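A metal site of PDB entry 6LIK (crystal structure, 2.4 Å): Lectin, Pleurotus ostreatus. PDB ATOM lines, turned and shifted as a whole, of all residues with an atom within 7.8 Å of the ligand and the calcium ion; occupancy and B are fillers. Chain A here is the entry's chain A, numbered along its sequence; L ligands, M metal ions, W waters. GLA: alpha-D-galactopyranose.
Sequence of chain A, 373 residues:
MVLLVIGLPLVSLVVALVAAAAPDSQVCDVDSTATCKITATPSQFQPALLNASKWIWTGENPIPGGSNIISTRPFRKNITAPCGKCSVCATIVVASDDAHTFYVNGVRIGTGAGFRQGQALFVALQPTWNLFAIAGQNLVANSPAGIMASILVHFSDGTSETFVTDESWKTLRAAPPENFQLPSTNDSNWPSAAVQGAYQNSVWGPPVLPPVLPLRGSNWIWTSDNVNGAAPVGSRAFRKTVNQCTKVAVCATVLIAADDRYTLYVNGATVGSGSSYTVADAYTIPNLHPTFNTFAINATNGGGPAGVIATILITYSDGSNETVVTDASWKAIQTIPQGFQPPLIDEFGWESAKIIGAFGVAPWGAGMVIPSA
The calcium ion is bound by OD2 of Asp 260 (2.4 Å).
The calcium ion is bound by O3 of the ligand, at 2.4 Å.
O4 of the ligand binds the calcium ion (2.4 Å).
O of Pro 305 binds the calcium ion (2.4 Å).
The calcium ion is bound by O of Gly 303.
The calcium ion is bound by OD1 of Asn 301 (2.6 Å).
The side-chain carboxylate (OD1) of Asp 259 binds the calcium ion (2.6 Å).
Tyr 277 touches the ligand (OH to C5, 3.5 Å).
Hydrophobic or aromatic side chains that line the ligand: Tyr 277 and Pro 305.
Five residues have an atom within 4 Å of the ligand: Asp 259, Asp 260, Tyr 277, Gly 303 and Pro 305.
Along chain A the residues within 4 Å of the ligand span positions 259 to 305.
Of the 22 residues printed, 5 come within 4 Å of the calcium ion.
Along chain A the residues within 4 Å of the calcium ion span positions 259 to 305.
The indole nitrogen of Trp 364 sits at hydrogen-bond distance from the side-chain carboxylate of Asp 259 (2.8 Å).
N of Asp 260 lies within hydrogen-bond range of O of Thr 300.
The side-chain carboxylate of Asp 260 sits close to the backbone NH of Gly 302 (2.9 Å).
The backbone carbonyl oxygen (O) of Pro 232 sits at hydrogen-bond distance from the side-chain amide nitrogen (ND2) of Asn 301.
O of Ala 231 lies within hydrogen-bond range of ND2 of Asn 301.
The side-chain amide nitrogen (ND2) of Asn 301 sits at hydrogen-bond distance from the backbone carbonyl oxygen (O) of Gly 304 (2.9 Å).
The backbone carbonyl oxygen of Gly 307 lies within hydrogen-bond range of the backbone NH of Asp 259, 2.8 Å away.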
ATOM      1  N   TRP A 222      32.366  -3.527 -31.356  1.00  0.00           N
ATOM      2  CA  TRP A 222      32.173  -3.813 -29.908  1.00  0.00           C
ATOM      3  C   TRP A 222      32.167  -5.334 -29.719  1.00  0.00           C
ATOM      4  O   TRP A 222      32.307  -6.079 -30.749  1.00  0.00           O
ATOM      5  CB  TRP A 222      30.894  -3.123 -29.430  1.00  0.00           C
ATOM      6  CG  TRP A 222      30.845  -2.820 -27.968  1.00  0.00           C
ATOM      7  CD1 TRP A 222      30.048  -3.447 -27.063  1.00  0.00           C
ATOM      8  CD2 TRP A 222      31.577  -1.818 -27.258  1.00  0.00           C
ATOM      9  NE1 TRP A 222      30.301  -2.945 -25.819  1.00  0.00           N
ATOM     10  CE2 TRP A 222      31.210  -1.926 -25.910  1.00  0.00           C
ATOM     11  CE3 TRP A 222      32.519  -0.861 -27.605  1.00  0.00           C
ATOM     12  CZ2 TRP A 222      31.727  -1.098 -24.920  1.00  0.00           C
ATOM     13  CZ3 TRP A 222      33.050  -0.050 -26.620  1.00  0.00           C
ATOM     14  CH2 TRP A 222      32.654  -0.169 -25.293  1.00  0.00           C
ATOM     15  N   GLY A 229      20.902  -1.337 -30.888  1.00  0.00           N
ATOM     16  CA  GLY A 229      21.468   0.026 -30.769  1.00  0.00           C
ATOM     17  C   GLY A 229      21.925   0.403 -29.361  1.00  0.00           C
ATOM     18  O   GLY A 229      22.147   1.615 -29.114  1.00  0.00           O
ATOM     19  N   ALA A 230      22.125  -0.559 -28.467  1.00  0.00           N
ATOM     20  CA  ALA A 230      22.645  -0.282 -27.109  1.00  0.00           C
ATOM     21  C   ALA A 230      23.515  -1.449 -26.637  1.00  0.00           C
ATOM     22  O   ALA A 230      23.415  -2.572 -27.200  1.00  0.00           O
ATOM     23  CB  ALA A 230      21.519   0.014 -26.129  1.00  0.00           C
ATOM     24  N   ALA A 231      24.346  -1.202 -25.626  1.00  0.00           N
ATOM     25  CA  ALA A 231      25.202  -2.262 -25.055  1.00  0.00           C
ATOM     26  C   ALA A 231      25.195  -2.096 -23.557  1.00  0.00           C
ATOM     27  O   ALA A 231      24.921  -1.000 -23.092  1.00  0.00           O
ATOM     28  CB  ALA A 231      26.604  -2.173 -25.573  1.00  0.00           C
ATOM     29  N   PRO A 232      25.508  -3.152 -22.776  1.00  0.00           N
ATOM     30  CA  PRO A 232      25.530  -3.031 -21.323  1.00  0.00           C
ATOM     31  C   PRO A 232      26.543  -1.960 -20.881  1.00  0.00           C
ATOM     32  O   PRO A 232      27.441  -1.642 -21.652  1.00  0.00           O
ATOM     33  CB  PRO A 232      25.880  -4.442 -20.849  1.00  0.00           C
ATOM     34  CG  PRO A 232      25.463  -5.354 -22.000  1.00  0.00           C
ATOM     35  CD  PRO A 232      25.711  -4.528 -23.245  1.00  0.00           C
ATOM     36  N   ALA A 258      36.074   6.646 -29.052  1.00  0.00           N
ATOM     37  CA  ALA A 258      35.219   5.633 -28.415  1.00  0.00           C
ATOM     38  C   ALA A 258      33.981   6.278 -27.817  1.00  0.00           C
ATOM     39  O   ALA A 258      34.090   7.361 -27.213  1.00  0.00           O
ATOM     40  CB  ALA A 258      36.011   4.916 -27.352  1.00  0.00           C
ATOM     41  N   ASP A 259      32.866   5.582 -27.921  1.00  0.00           N
ATOM     42  CA  ASP A 259      31.650   5.859 -27.148  1.00  0.00           C
ATOM     43  C   ASP A 259      31.591   4.920 -25.922  1.00  0.00           C
ATOM     44  O   ASP A 259      31.283   3.729 -26.117  1.00  0.00           O
ATOM     45  CB  ASP A 259      30.404   5.726 -28.022  1.00  0.00           C
ATOM     46  CG  ASP A 259      29.127   6.136 -27.284  1.00  0.00           C
ATOM     47  OD1 ASP A 259      29.231   6.301 -26.052  1.00  0.00           O
ATOM     48  OD2 ASP A 259      28.069   6.311 -27.960  1.00  0.00           O
ATOM     49  N   ASP A 260      32.347   5.322 -24.919  1.00  0.00           N
ATOM     50  CA  ASP A 260      32.189   6.552 -24.097  1.00  0.00           C
ATOM     51  C   ASP A 260      33.616   7.047 -23.886  1.00  0.00           C
ATOM     52  O   ASP A 260      33.794   8.263 -23.935  1.00  0.00           O
ATOM     53  CB  ASP A 260      31.396   6.374 -22.802  1.00  0.00           C
ATOM     54  CG  ASP A 260      29.925   6.758 -22.977  1.00  0.00           C
ATOM     55  OD1 ASP A 260      29.674   7.962 -23.302  1.00  0.00           O
ATOM     56  OD2 ASP A 260      29.055   5.842 -22.883  1.00  0.00           O
ATOM     57  N   ARG A 261      34.593   6.120 -23.837  1.00  0.00           N
ATOM     58  CA  ARG A 261      35.923   6.285 -23.176  1.00  0.00           C
ATOM     59  C   ARG A 261      36.829   5.114 -23.627  1.00  0.00           C
ATOM     60  O   ARG A 261      36.295   4.012 -23.951  1.00  0.00           O
ATOM     61  CB  ARG A 261      35.593   6.378 -21.677  1.00  0.00           C
ATOM     62  CG  ARG A 261      36.677   6.006 -20.670  1.00  0.00           C
ATOM     63  CD  ARG A 261      36.112   5.910 -19.255  1.00  0.00           C
ATOM     64  NE  ARG A 261      35.081   6.907 -18.973  1.00  0.00           N
ATOM     65  CZ  ARG A 261      35.303   8.209 -18.746  1.00  0.00           C
ATOM     66  NH1 ARG A 261      36.533   8.708 -18.759  1.00  0.00           N
ATOM     67  NH2 ARG A 261      34.272   9.020 -18.521  1.00  0.00           N
ATOM     68  N   TYR A 277      33.364  10.845 -28.169  1.00  0.00           N
ATOM     69  CA  TYR A 277      32.949  10.196 -29.431  1.00  0.00           C
ATOM     70  C   TYR A 277      32.645  11.248 -30.513  1.00  0.00           C
ATOM     71  O   TYR A 277      32.181  10.822 -31.581  1.00  0.00           O
ATOM     72  CB  TYR A 277      31.782   9.237 -29.185  1.00  0.00           C
ATOM     73  CG  TYR A 277      30.579   9.822 -28.490  1.00  0.00           C
ATOM     74  CD1 TYR A 277      29.593  10.451 -29.222  1.00  0.00           C
ATOM     75  CD2 TYR A 277      30.412   9.689 -27.119  1.00  0.00           C
ATOM     76  CE1 TYR A 277      28.468  10.961 -28.613  1.00  0.00           C
ATOM     77  CE2 TYR A 277      29.288  10.194 -26.490  1.00  0.00           C
ATOM     78  CZ  TYR A 277      28.311  10.830 -27.242  1.00  0.00           C
ATOM     79  OH  TYR A 277      27.185  11.342 -26.683  1.00  0.00           O
ATOM     80  N   THR A 278      32.943  12.534 -30.283  1.00  0.00           N
ATOM     81  CA  THR A 278      32.777  13.609 -31.296  1.00  0.00           C
ATOM     82  C   THR A 278      34.138  14.249 -31.654  1.00  0.00           C
ATOM     83  O   THR A 278      34.211  14.856 -32.736  1.00  0.00           O
ATOM     84  CB  THR A 278      31.807  14.706 -30.818  1.00  0.00           C
ATOM     85  OG1 THR A 278      32.261  15.182 -29.551  1.00  0.00           O
ATOM     86  CG2 THR A 278      30.372  14.251 -30.667  1.00  0.00           C
ATOM     87  N   THR A 300      35.077   1.711 -22.507  1.00  0.00           N
ATOM     88  CA  THR A 300      34.009   1.657 -21.474  1.00  0.00           C
ATOM     89  C   THR A 300      32.731   2.316 -22.005  1.00  0.00           C
ATOM     90  O   THR A 300      32.809   3.415 -22.542  1.00  0.00           O
ATOM     91  CB  THR A 300      34.538   2.302 -20.180  1.00  0.00           C
ATOM     92  OG1 THR A 300      35.733   1.650 -19.745  1.00  0.00           O
ATOM     93  CG2 THR A 300      33.525   2.237 -19.060  1.00  0.00           C
ATOM     94  N   ASN A 301      31.594   1.632 -21.858  1.00  0.00           N
ATOM     95  CA  ASN A 301      30.239   2.185 -22.049  1.00  0.00           C
ATOM     96  C   ASN A 301      29.663   2.688 -20.711  1.00  0.00           C
ATOM     97  O   ASN A 301      29.499   1.890 -19.785  1.00  0.00           O
ATOM     98  CB  ASN A 301      29.286   1.164 -22.637  1.00  0.00           C
ATOM     99  CG  ASN A 301      27.975   1.786 -23.093  1.00  0.00           C
ATOM    100  OD1 ASN A 301      27.930   2.989 -23.245  1.00  0.00           O
ATOM    101  ND2 ASN A 301      26.921   0.999 -23.286  1.00  0.00           N
ATOM    102  N   GLY A 302      29.361   3.988 -20.638  1.00  0.00           N
ATOM    103  CA  GLY A 302      28.631   4.625 -19.536  1.00  0.00           C
ATOM    104  C   GLY A 302      27.127   4.382 -19.607  1.00  0.00           C
ATOM    105  O   GLY A 302      26.465   4.708 -18.628  1.00  0.00           O
ATOM    106  N   GLY A 303      26.604   3.894 -20.728  1.00  0.00           N
ATOM    107  CA  GLY A 303      25.159   3.661 -20.945  1.00  0.00           C
ATOM    108  C   GLY A 303      24.755   4.007 -22.362  1.00  0.00           C
ATOM    109  O   GLY A 303      25.356   4.923 -22.924  1.00  0.00           O
ATOM    110  N   GLY A 304      23.799   3.277 -22.928  1.00  0.00           N
ATOM    111  CA  GLY A 304      23.279   3.504 -24.275  1.00  0.00           C
ATOM    112  C   GLY A 304      24.159   2.843 -25.319  1.00  0.00           C
ATOM    113  O   GLY A 304      24.805   1.842 -25.030  1.00  0.00           O
ATOM    114  N   PRO A 305      24.214   3.385 -26.571  1.00  0.00           N
ATOM    115  CA  PRO A 305      25.081   2.873 -27.630  1.00  0.00           C
ATOM    116  C   PRO A 305      26.557   2.885 -27.191  1.00  0.00           C
ATOM    117  O   PRO A 305      26.958   3.633 -26.276  1.00  0.00           O
ATOM    118  CB  PRO A 305      24.885   3.855 -28.798  1.00  0.00           C
ATOM    119  CG  PRO A 305      23.585   4.541 -28.526  1.00  0.00           C
ATOM    120  CD  PRO A 305      23.518   4.604 -27.009  1.00  0.00           C
ATOM    121  N   ALA A 306      27.342   2.061 -27.858  1.00  0.00           N
ATOM    122  CA  ALA A 306      28.784   1.945 -27.563  1.00  0.00           C
ATOM    123  C   ALA A 306      29.536   1.532 -28.817  1.00  0.00           C
ATOM    124  O   ALA A 306      28.967   0.799 -29.687  1.00  0.00           O
ATOM    125  CB  ALA A 306      28.983   0.949 -26.461  1.00  0.00           C
ATOM    126  N   GLY A 307      30.787   1.935 -28.887  1.00  0.00           N
ATOM    127  CA  GLY A 307      31.634   1.466 -30.006  1.00  0.00           C
ATOM    128  C   GLY A 307      33.022   2.045 -29.906  1.00  0.00           C
ATOM    129  O   GLY A 307      33.226   3.071 -29.209  1.00  0.00           O
ATOM    130  N   ALA A 362      24.527   6.076 -37.917  1.00  0.00           N
ATOM    131  CA  ALA A 362      23.857   6.495 -36.656  1.00  0.00           C
ATOM    132  C   ALA A 362      24.292   5.541 -35.558  1.00  0.00           C
ATOM    133  O   ALA A 362      24.488   4.341 -35.776  1.00  0.00           O
ATOM    134  CB  ALA A 362      22.358   6.408 -36.833  1.00  0.00           C
ATOM    135  N   PRO A 363      24.324   5.983 -34.314  1.00  0.00           N
ATOM    136  CA  PRO A 363      23.966   7.357 -33.970  1.00  0.00           C
ATOM    137  C   PRO A 363      25.049   8.421 -34.123  1.00  0.00           C
ATOM    138  O   PRO A 363      24.753   9.566 -33.861  1.00  0.00           O
ATOM    139  CB  PRO A 363      23.640   7.250 -32.470  1.00  0.00           C
ATOM    140  CG  PRO A 363      24.486   6.097 -31.994  1.00  0.00           C
ATOM    141  CD  PRO A 363      24.515   5.116 -33.148  1.00  0.00           C
ATOM    142  N   TRP A 364      26.281   8.038 -34.398  1.00  0.00           N
ATOM    143  CA  TRP A 364      27.425   8.972 -34.288  1.00  0.00           C
ATOM    144  C   TRP A 364      27.537   9.809 -35.563  1.00  0.00           C
ATOM    145  O   TRP A 364      27.969  10.904 -35.420  1.00  0.00           O
ATOM    146  CB  TRP A 364      28.735   8.213 -33.990  1.00  0.00           C
ATOM    147  CG  TRP A 364      28.586   7.307 -32.802  1.00  0.00           C
ATOM    148  CD1 TRP A 364      28.547   7.651 -31.486  1.00  0.00           C
ATOM    149  CD2 TRP A 364      28.416   5.868 -32.861  1.00  0.00           C
ATOM    150  NE1 TRP A 364      28.333   6.524 -30.721  1.00  0.00           N
ATOM    151  CE2 TRP A 364      28.277   5.426 -31.538  1.00  0.00           C
ATOM    152  CE3 TRP A 364      28.376   4.923 -33.889  1.00  0.00           C
ATOM    153  CZ2 TRP A 364      28.090   4.077 -31.233  1.00  0.00           C
ATOM    154  CZ3 TRP A 364      28.205   3.590 -33.591  1.00  0.00           C
ATOM    155  CH2 TRP A 364      28.081   3.174 -32.272  1.00  0.00           C
HETATM  156  C1  GLA L   1      23.681   8.192 -24.588  1.00  0.00           C
HETATM  157  C2  GLA L   1      24.970   8.408 -23.674  1.00  0.00           C
HETATM  158  C3  GLA L   1      26.282   8.479 -24.522  1.00  0.00           C
HETATM  159  C4  GLA L   1      26.114   8.088 -26.034  1.00  0.00           C
HETATM  160  C5  GLA L   1      24.838   8.778 -26.723  1.00  0.00           C
HETATM  161  C6  GLA L   1      24.411   8.268 -28.124  1.00  0.00           C
HETATM  162  O1  GLA L   1      22.447   8.455 -23.899  1.00  0.00           O
HETATM  163  O2  GLA L   1      24.959   9.443 -22.631  1.00  0.00           O
HETATM  164  O3  GLA L   1      27.238   7.566 -23.900  1.00  0.00           O
HETATM  165  O4  GLA L   1      26.259   6.617 -26.110  1.00  0.00           O
HETATM  166  O5  GLA L   1      23.630   8.842 -25.899  1.00  0.00           O
HETATM  167  O6  GLA L   1      25.087   8.976 -29.156  1.00  0.00           O
HETATM  168 CA    CA M   1      27.412   5.222 -24.494  1.00  0.00          CA
HETATM  169  O   HOH W   1      26.716   7.501 -21.076  1.00  0.00           O
